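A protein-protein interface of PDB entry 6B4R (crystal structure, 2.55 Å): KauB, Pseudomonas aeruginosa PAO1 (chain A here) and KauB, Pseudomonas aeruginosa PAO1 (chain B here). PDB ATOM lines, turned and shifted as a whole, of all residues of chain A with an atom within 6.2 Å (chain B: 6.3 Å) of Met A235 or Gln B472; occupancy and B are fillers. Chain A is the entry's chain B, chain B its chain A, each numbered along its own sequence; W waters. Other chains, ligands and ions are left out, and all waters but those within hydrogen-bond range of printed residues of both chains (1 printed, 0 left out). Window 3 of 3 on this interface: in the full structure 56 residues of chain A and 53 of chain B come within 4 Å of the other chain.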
ATOM      1  N   ALA A 230      -0.284  38.534 -30.385  1.00  0.00           N
ATOM      2  CA  ALA A 230       0.877  38.154 -29.583  1.00  0.00           C
ATOM      3  C   ALA A 230       0.549  38.154 -28.094  1.00  0.00           C
ATOM      4  O   ALA A 230       0.994  37.278 -27.353  1.00  0.00           O
ATOM      5  CB  ALA A 230       2.049  39.084 -29.869  1.00  0.00           C
ATOM      6  N   LEU A 231      -0.224  39.145 -27.662  1.00  0.00           N
ATOM      7  CA  LEU A 231      -0.657  39.229 -26.273  1.00  0.00           C
ATOM      8  C   LEU A 231      -1.625  38.095 -25.946  1.00  0.00           C
ATOM      9  O   LEU A 231      -1.564  37.505 -24.866  1.00  0.00           O
ATOM     10  CB  LEU A 231      -1.314  40.584 -25.997  1.00  0.00           C
ATOM     11  CG  LEU A 231      -0.395  41.807 -26.036  1.00  0.00           C
ATOM     12  CD1 LEU A 231      -1.200  43.094 -26.009  1.00  0.00           C
ATOM     13  CD2 LEU A 231       0.581  41.767 -24.876  1.00  0.00           C
ATOM     14  N   LEU A 233      -1.705  35.217 -27.291  1.00  0.00           N
ATOM     15  CA  LEU A 233      -1.012  33.934 -27.345  1.00  0.00           C
ATOM     16  C   LEU A 233       0.128  33.842 -26.339  1.00  0.00           C
ATOM     17  O   LEU A 233       0.749  32.790 -26.192  1.00  0.00           O
ATOM     18  CB  LEU A 233      -0.486  33.665 -28.758  1.00  0.00           C
ATOM     19  CG  LEU A 233      -1.518  33.176 -29.776  1.00  0.00           C
ATOM     20  CD1 LEU A 233      -0.971  33.273 -31.191  1.00  0.00           C
ATOM     21  CD2 LEU A 233      -1.933  31.747 -29.458  1.00  0.00           C
ATOM     22  N   HIS A 234       0.401  34.939 -25.642  1.00  0.00           N
ATOM     23  CA  HIS A 234       1.528  34.970 -24.716  1.00  0.00           C
ATOM     24  C   HIS A 234       1.301  34.046 -23.520  1.00  0.00           C
ATOM     25  O   HIS A 234       0.213  34.008 -22.949  1.00  0.00           O
ATOM     26  CB  HIS A 234       1.813  36.397 -24.250  1.00  0.00           C
ATOM     27  CG  HIS A 234       3.209  36.595 -23.749  1.00  0.00           C
ATOM     28  ND1 HIS A 234       3.621  36.175 -22.503  1.00  0.00           N
ATOM     29  CD2 HIS A 234       4.292  37.162 -24.331  1.00  0.00           C
ATOM     30  CE1 HIS A 234       4.896  36.476 -22.337  1.00  0.00           C
ATOM     31  NE2 HIS A 234       5.327  37.077 -23.432  1.00  0.00           N
ATOM     32  N   MET A 235       2.341  33.304 -23.147  1.00  0.00           N
ATOM     33  CA  MET A 235       2.229  32.287 -22.104  1.00  0.00           C
ATOM     34  C   MET A 235       2.268  32.845 -20.681  1.00  0.00           C
ATOM     35  O   MET A 235       2.015  32.115 -19.722  1.00  0.00           O
ATOM     36  CB  MET A 235       3.327  31.229 -22.273  1.00  0.00           C
ATOM     37  CG  MET A 235       3.213  30.402 -23.547  1.00  0.00           C
ATOM     38  SD  MET A 235       1.692  29.432 -23.640  1.00  0.00           S
ATOM     39  CE  MET A 235       1.934  28.267 -22.302  1.00  0.00           C
ATOM     40  N   ASP A 236       2.588  34.131 -20.544  1.00  0.00           N
ATOM     41  CA  ASP A 236       2.726  34.744 -19.222  1.00  0.00           C
ATOM     42  C   ASP A 236       1.695  35.852 -18.981  1.00  0.00           C
ATOM     43  O   ASP A 236       1.814  36.627 -18.030  1.00  0.00           O
ATOM     44  CB  ASP A 236       4.151  35.279 -19.017  1.00  0.00           C
ATOM     45  CG  ASP A 236       4.499  35.486 -17.546  1.00  0.00           C
ATOM     46  OD1 ASP A 236       4.148  34.628 -16.707  1.00  0.00           O
ATOM     47  OD2 ASP A 236       5.122  36.517 -17.228  1.00  0.00           O
ATOM     48  N   VAL A 237       0.690  35.926 -19.848  1.00  0.00           N
ATOM     49  CA  VAL A 237      -0.434  36.835 -19.635  1.00  0.00           C
ATOM     50  C   VAL A 237      -1.558  36.096 -18.919  1.00  0.00           C
ATOM     51  O   VAL A 237      -2.080  35.105 -19.429  1.00  0.00           O
ATOM     52  CB  VAL A 237      -0.966  37.418 -20.955  1.00  0.00           C
ATOM     53  CG1 VAL A 237      -2.245  38.212 -20.708  1.00  0.00           C
ATOM     54  CG2 VAL A 237       0.090  38.288 -21.613  1.00  0.00           C
ATOM     55  N   GLU A 258      -5.153  27.833 -27.102  1.00  0.00           N
ATOM     56  CA  GLU A 258      -3.934  27.335 -27.728  1.00  0.00           C
ATOM     57  C   GLU A 258      -2.701  27.647 -26.891  1.00  0.00           C
ATOM     58  O   GLU A 258      -1.676  26.980 -27.016  1.00  0.00           O
ATOM     59  CB  GLU A 258      -3.773  27.925 -29.130  1.00  0.00           C
ATOM     60  CG  GLU A 258      -4.804  27.425 -30.126  1.00  0.00           C
ATOM     61  CD  GLU A 258      -4.758  28.176 -31.438  1.00  0.00           C
ATOM     62  OE1 GLU A 258      -4.062  29.211 -31.508  1.00  0.00           O
ATOM     63  OE2 GLU A 258      -5.418  27.732 -32.402  1.00  0.00           O
ATOM     64  N   SER A 259      -2.805  28.659 -26.036  1.00  0.00           N
ATOM     65  CA  SER A 259      -1.657  29.103 -25.251  1.00  0.00           C
ATOM     66  C   SER A 259      -1.669  28.571 -23.819  1.00  0.00           C
ATOM     67  O   SER A 259      -1.358  27.406 -23.580  1.00  0.00           O
ATOM     68  CB  SER A 259      -1.561  30.632 -25.251  1.00  0.00           C
ATOM     69  OG  SER A 259      -2.743  31.227 -24.745  1.00  0.00           O
ATOM     70  N   ASN A 260      -2.023  29.430 -22.870  1.00  0.00           N
ATOM     71  CA  ASN A 260      -1.919  29.074 -21.460  1.00  0.00           C
ATOM     72  C   ASN A 260      -3.258  29.039 -20.733  1.00  0.00           C
ATOM     73  O   ASN A 260      -3.296  29.092 -19.503  1.00  0.00           O
ATOM     74  CB  ASN A 260      -0.967  30.034 -20.746  1.00  0.00           C
ATOM     75  CG  ASN A 260      -1.498  31.450 -20.697  1.00  0.00           C
ATOM     76  OD1 ASN A 260      -2.384  31.823 -21.468  1.00  0.00           O
ATOM     77  ND2 ASN A 260      -0.954  32.252 -19.791  1.00  0.00           N
ATOM     78  N   MET A 261      -4.343  28.958 -21.498  1.00  0.00           N
ATOM     79  CA  MET A 261      -5.692  28.868 -20.942  1.00  0.00           C
ATOM     80  C   MET A 261      -6.028  30.102 -20.103  1.00  0.00           C
ATOM     81  O   MET A 261      -6.734  30.013 -19.098  1.00  0.00           O
ATOM     82  CB  MET A 261      -5.832  27.594 -20.102  1.00  0.00           C
ATOM     83  CG  MET A 261      -7.213  26.973 -20.097  1.00  0.00           C
ATOM     84  SD  MET A 261      -7.341  25.713 -18.814  1.00  0.00           S
ATOM     85  CE  MET A 261      -5.829  24.806 -19.086  1.00  0.00           C
ATOM     86  N   LYS A 262      -5.505  31.251 -20.519  1.00  0.00           N
ATOM     87  CA  LYS A 262      -5.717  32.502 -19.801  1.00  0.00           C
ATOM     88  C   LYS A 262      -7.202  32.849 -19.738  1.00  0.00           C
ATOM     89  O   LYS A 262      -7.971  32.474 -20.623  1.00  0.00           O
ATOM     90  CB  LYS A 262      -4.939  33.640 -20.470  1.00  0.00           C
ATOM     91  CG  LYS A 262      -5.303  33.870 -21.932  1.00  0.00           C
ATOM     92  CD  LYS A 262      -4.616  35.109 -22.502  1.00  0.00           C
ATOM     93  CE  LYS A 262      -3.106  34.926 -22.599  1.00  0.00           C
ATOM     94  NZ  LYS A 262      -2.740  33.815 -23.525  1.00  0.00           N
ATOM     95  N   ARG A 263      -7.601  33.556 -18.684  1.00  0.00           N
ATOM     96  CA  ARG A 263      -8.986  33.991 -18.540  1.00  0.00           C
ATOM     97  C   ARG A 263      -9.327  35.001 -19.622  1.00  0.00           C
ATOM     98  O   ARG A 263      -8.573  35.943 -19.863  1.00  0.00           O
ATOM     99  CB  ARG A 263      -9.237  34.608 -17.162  1.00  0.00           C
ATOM    100  CG  ARG A 263      -9.144  33.631 -16.003  1.00  0.00           C
ATOM    101  CD  ARG A 263      -7.727  33.545 -15.462  1.00  0.00           C
ATOM    102  NE  ARG A 263      -7.638  32.665 -14.302  1.00  0.00           N
ATOM    103  CZ  ARG A 263      -7.352  31.369 -14.370  1.00  0.00           C
ATOM    104  NH1 ARG A 263      -7.127  30.798 -15.546  1.00  0.00           N
ATOM    105  NH2 ARG A 263      -7.290  30.646 -13.261  1.00  0.00           N
ATOM    106  N   THR B 246      -5.349  19.354 -18.196  1.00  0.00           N
ATOM    107  CA  THR B 246      -5.059  20.655 -18.787  1.00  0.00           C
ATOM    108  C   THR B 246      -5.173  20.617 -20.310  1.00  0.00           C
ATOM    109  O   THR B 246      -5.691  21.549 -20.927  1.00  0.00           O
ATOM    110  CB  THR B 246      -3.651  21.138 -18.377  1.00  0.00           C
ATOM    111  OG1 THR B 246      -3.639  21.426 -16.972  1.00  0.00           O
ATOM    112  CG2 THR B 246      -3.253  22.387 -19.142  1.00  0.00           C
ATOM    113  N   LYS B 250      -7.900  22.849 -22.412  1.00  0.00           N
ATOM    114  CA  LYS B 250      -7.491  23.794 -23.441  1.00  0.00           C
ATOM    115  C   LYS B 250      -8.262  23.542 -24.731  1.00  0.00           C
ATOM    116  O   LYS B 250      -8.710  24.478 -25.390  1.00  0.00           O
ATOM    117  CB  LYS B 250      -5.989  23.683 -23.703  1.00  0.00           C
ATOM    118  CG  LYS B 250      -5.105  24.308 -22.641  1.00  0.00           C
ATOM    119  CD  LYS B 250      -3.634  24.123 -22.989  1.00  0.00           C
ATOM    120  CE  LYS B 250      -2.727  24.729 -21.929  1.00  0.00           C
ATOM    121  NZ  LYS B 250      -1.290  24.458 -22.219  1.00  0.00           N
ATOM    122  N   GLU B 267     -11.682  23.010 -14.527  1.00  0.00           N
ATOM    123  CA  GLU B 267     -10.832  22.645 -13.403  1.00  0.00           C
ATOM    124  C   GLU B 267      -9.811  21.618 -13.880  1.00  0.00           C
ATOM    125  O   GLU B 267     -10.111  20.428 -13.964  1.00  0.00           O
ATOM    126  CB  GLU B 267     -11.668  22.082 -12.251  1.00  0.00           C
ATOM    127  CG  GLU B 267     -12.847  22.964 -11.858  1.00  0.00           C
ATOM    128  CD  GLU B 267     -12.991  23.119 -10.356  1.00  0.00           C
ATOM    129  OE1 GLU B 267     -12.469  22.261  -9.614  1.00  0.00           O
ATOM    130  OE2 GLU B 267     -13.620  24.105  -9.917  1.00  0.00           O
ATOM    131  N   ALA B 268      -8.608  22.083 -14.205  1.00  0.00           N
ATOM    132  CA  ALA B 268      -7.595  21.227 -14.813  1.00  0.00           C
ATOM    133  C   ALA B 268      -6.697  20.516 -13.803  1.00  0.00           C
ATOM    134  O   ALA B 268      -7.072  20.317 -12.647  1.00  0.00           O
ATOM    135  CB  ALA B 268      -6.762  22.019 -15.813  1.00  0.00           C
ATOM    136  N   GLY B 269      -5.509  20.131 -14.253  1.00  0.00           N
ATOM    137  CA  GLY B 269      -4.595  19.366 -13.429  1.00  0.00           C
ATOM    138  C   GLY B 269      -3.972  20.175 -12.309  1.00  0.00           C
ATOM    139  O   GLY B 269      -4.283  21.353 -12.123  1.00  0.00           O
ATOM    140  N   PRO B 426       3.206  25.538 -13.573  1.00  0.00           N
ATOM    141  CA  PRO B 426       2.140  26.100 -14.408  1.00  0.00           C
ATOM    142  C   PRO B 426       0.772  25.966 -13.737  1.00  0.00           C
ATOM    143  O   PRO B 426      -0.186  26.622 -14.148  1.00  0.00           O
ATOM    144  CB  PRO B 426       2.200  25.241 -15.674  1.00  0.00           C
ATOM    145  CG  PRO B 426       2.807  23.955 -15.233  1.00  0.00           C
ATOM    146  CD  PRO B 426       3.799  24.327 -14.170  1.00  0.00           C
ATOM    147  N   TYR B 427       0.694  25.134 -12.704  1.00  0.00           N
ATOM    148  CA  TYR B 427      -0.555  24.900 -11.991  1.00  0.00           C
ATOM    149  C   TYR B 427      -0.719  25.824 -10.781  1.00  0.00           C
ATOM    150  O   TYR B 427       0.122  26.686 -10.519  1.00  0.00           O
ATOM    151  CB  TYR B 427      -0.638  23.440 -11.540  1.00  0.00           C
ATOM    152  CG  TYR B 427      -0.564  22.427 -12.665  1.00  0.00           C
ATOM    153  CD1 TYR B 427      -1.591  22.320 -13.594  1.00  0.00           C
ATOM    154  CD2 TYR B 427       0.521  21.562 -12.782  1.00  0.00           C
ATOM    155  CE1 TYR B 427      -1.539  21.393 -14.613  1.00  0.00           C
ATOM    156  CE2 TYR B 427       0.581  20.626 -13.801  1.00  0.00           C
ATOM    157  CZ  TYR B 427      -0.455  20.549 -14.713  1.00  0.00           C
ATOM    158  OH  TYR B 427      -0.411  19.625 -15.730  1.00  0.00           O
ATOM    159  N   GLY B 428      -1.805  25.626 -10.041  1.00  0.00           N
ATOM    160  CA  GLY B 428      -2.106  26.432  -8.871  1.00  0.00           C
ATOM    161  C   GLY B 428      -3.478  26.104  -8.307  1.00  0.00           C
ATOM    162  O   GLY B 428      -4.306  26.985  -8.077  1.00  0.00           O
ATOM    163  N   GLY B 469      -8.801  26.504  -9.455  1.00  0.00           N
ATOM    164  CA  GLY B 469      -7.379  26.745  -9.620  1.00  0.00           C
ATOM    165  C   GLY B 469      -6.958  28.132 -10.068  1.00  0.00           C
ATOM    166  O   GLY B 469      -7.752  28.893 -10.617  1.00  0.00           O
ATOM    167  N   PHE B 470      -5.697  28.464  -9.803  1.00  0.00           N
ATOM    168  CA  PHE B 470      -5.049  29.619 -10.408  1.00  0.00           C
ATOM    169  C   PHE B 470      -4.424  29.140 -11.706  1.00  0.00           C
ATOM    170  O   PHE B 470      -4.175  27.945 -11.869  1.00  0.00           O
ATOM    171  CB  PHE B 470      -3.937  30.157  -9.503  1.00  0.00           C
ATOM    172  CG  PHE B 470      -4.418  31.049  -8.391  1.00  0.00           C
ATOM    173  CD1 PHE B 470      -5.517  30.701  -7.618  1.00  0.00           C
ATOM    174  CD2 PHE B 470      -3.746  32.225  -8.098  1.00  0.00           C
ATOM    175  CE1 PHE B 470      -5.949  31.522  -6.587  1.00  0.00           C
ATOM    176  CE2 PHE B 470      -4.169  33.049  -7.069  1.00  0.00           C
ATOM    177  CZ  PHE B 470      -5.271  32.696  -6.310  1.00  0.00           C
ATOM    178  N   LYS B 471      -4.170  30.072 -12.619  1.00  0.00           N
ATOM    179  CA  LYS B 471      -3.429  29.789 -13.849  1.00  0.00           C
ATOM    180  C   LYS B 471      -3.993  28.618 -14.662  1.00  0.00           C
ATOM    181  O   LYS B 471      -5.161  28.627 -15.048  1.00  0.00           O
ATOM    182  CB  LYS B 471      -1.944  29.576 -13.537  1.00  0.00           C
ATOM    183  CG  LYS B 471      -1.276  30.796 -12.917  1.00  0.00           C
ATOM    184  CD  LYS B 471       0.229  30.618 -12.779  1.00  0.00           C
ATOM    185  CE  LYS B 471       0.578  29.631 -11.681  1.00  0.00           C
ATOM    186  NZ  LYS B 471       2.051  29.527 -11.484  1.00  0.00           N
ATOM    187  N   GLN B 472      -3.162  27.610 -14.916  1.00  0.00           N
ATOM    188  CA  GLN B 472      -3.563  26.494 -15.768  1.00  0.00           C
ATOM    189  C   GLN B 472      -4.263  25.370 -15.007  1.00  0.00           C
ATOM    190  O   GLN B 472      -4.490  24.292 -15.554  1.00  0.00           O
ATOM    191  CB  GLN B 472      -2.367  25.944 -16.552  1.00  0.00           C
ATOM    192  CG  GLN B 472      -1.768  26.940 -17.531  1.00  0.00           C
ATOM    193  CD  GLN B 472      -0.900  26.278 -18.584  1.00  0.00           C
ATOM    194  OE1 GLN B 472      -1.115  25.120 -18.944  1.00  0.00           O
ATOM    195  NE2 GLN B 472       0.088  27.011 -19.083  1.00  0.00           N
ATOM    196  N   SER B 473      -4.607  25.623 -13.749  1.00  0.00           N
ATOM    197  CA  SER B 473      -5.394  24.667 -12.975  1.00  0.00           C
ATOM    198  C   SER B 473      -6.883  24.901 -13.199  1.00  0.00           C
ATOM    199  O   SER B 473      -7.727  24.195 -12.649  1.00  0.00           O
ATOM    200  CB  SER B 473      -5.055  24.748 -11.484  1.00  0.00           C
ATOM    201  OG  SER B 473      -3.828  24.097 -11.199  1.00  0.00           O
ATOM    202  N   GLY B 474      -7.196  25.903 -14.013  1.00  0.00           N
ATOM    203  CA  GLY B 474      -8.569  26.172 -14.393  1.00  0.00           C
ATOM    204  C   GLY B 474      -9.052  27.558 -14.014  1.00  0.00           C
ATOM    205  O   GLY B 474      -8.282  28.385 -13.528  1.00  0.00           O
HETATM  206  O   HOH W   1      -3.228  30.629 -17.145  1.00  0.00           O
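The side-chain amino group (NZ) of Lys B250 lies within hydrogen-bond range of the backbone carbonyl oxygen (O) of Ser A259, at 3.2 Å. The guanidinium group of Arg A263 lies within hydrogen-bond range of the backbone carbonyl oxygen of Gly B474, 2.5 Å away. The guanidinium group (NH1) of Arg A263 is in hydrogen-bond range of the backbone carbonyl oxygen (O) of Lys B471, at 3.0 Å. The guanidinium group of Arg A263 is in hydrogen-bond range of the backbone carbonyl oxygen of Gly B469 (3.2 Å).
O of Gly B428 lies within hydrogen-bond range of N of Phe B470 (2.7 Å). OD1 of Asn A260 is in hydrogen-bond range of NZ of Lys A262. The backbone carbonyl oxygen (O) of Met A235 is in hydrogen-bond range of the side-chain amide nitrogen (ND2) of Asn A260 (3.0 Å). OG1 of Thr B246 is in hydrogen-bond range of O of Gln B472 (3.3 Å). The backbone carbonyl oxygen (O) of Pro B426 is in hydrogen-bond range of the backbone NH (N) of Gln B472, at 3.2 Å. The side-chain amino group (NZ) of Lys A262 is in hydrogen-bond range of the side-chain hydroxyl (OG) of Ser A259, 2.9 Å away.
NE2 of Gln B472 touches CE of Met A235, at 3.9 Å. CG of Gln B472 touches O of Asn A260, at 3.3 Å. CE of Met A261 touches CG2 of Thr B246, 3.5 Å away. Lys B250 touches Met A261 (CG to CE, 3.7 Å). CE of Met A261 touches O of Gln B472, 3.8 Å away. NH2 of Arg A263 touches C of Phe B470 (3.6 Å).
Of the printed residues of chain B, Met A235 touches Gln B472 (3.9 Å). Of the printed residues of chain A, Thr B246 touches Met A261. Of the printed residues of chain B, Met A261 touches Thr B246, Lys B250 and Gln B472. Printed residues of chain A within 4 Å of Phe B470: Arg A263 (3.6 Å). Of the printed residues of chain B, Arg A263 touches Gly B469 (3.2 Å), Phe B470 (3.6 Å), Lys B471 (3.0 Å) and Gly B474 (2.5 Å). Printed residues of chain A within 4 Å of Gly B474: Arg A263. Asp A236 touches none of the printed residues of chain B. Leu A231 touches none of the printed residues of chain B. The nearest residue of chain B that does not touch Met A235 is Lys B250 (5.0 Å). The nearest printed residue of chain B that does not touch Met A261 is Ala B268 (4.4 Å).
Printed residues of chain B that touch a printed residue of chain A: Thr B246, Lys B250, Gly B469, Phe B470, Lys B471, Gln B472 and Gly B474. Of the 13 printed residues of chain A, 5 touch a printed residue of chain B. Hydrophobic or aromatic side chains of chain A within 4 Å of the printed part of chain B: Met A235 and Met A261. Among the printed residues, no Asp or Glu carboxylate lies within 4 Å of a Lys or Arg side-chain nitrogen of the other chain.
Water W1 bridges O of Asn A260 and O of Lys B471.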
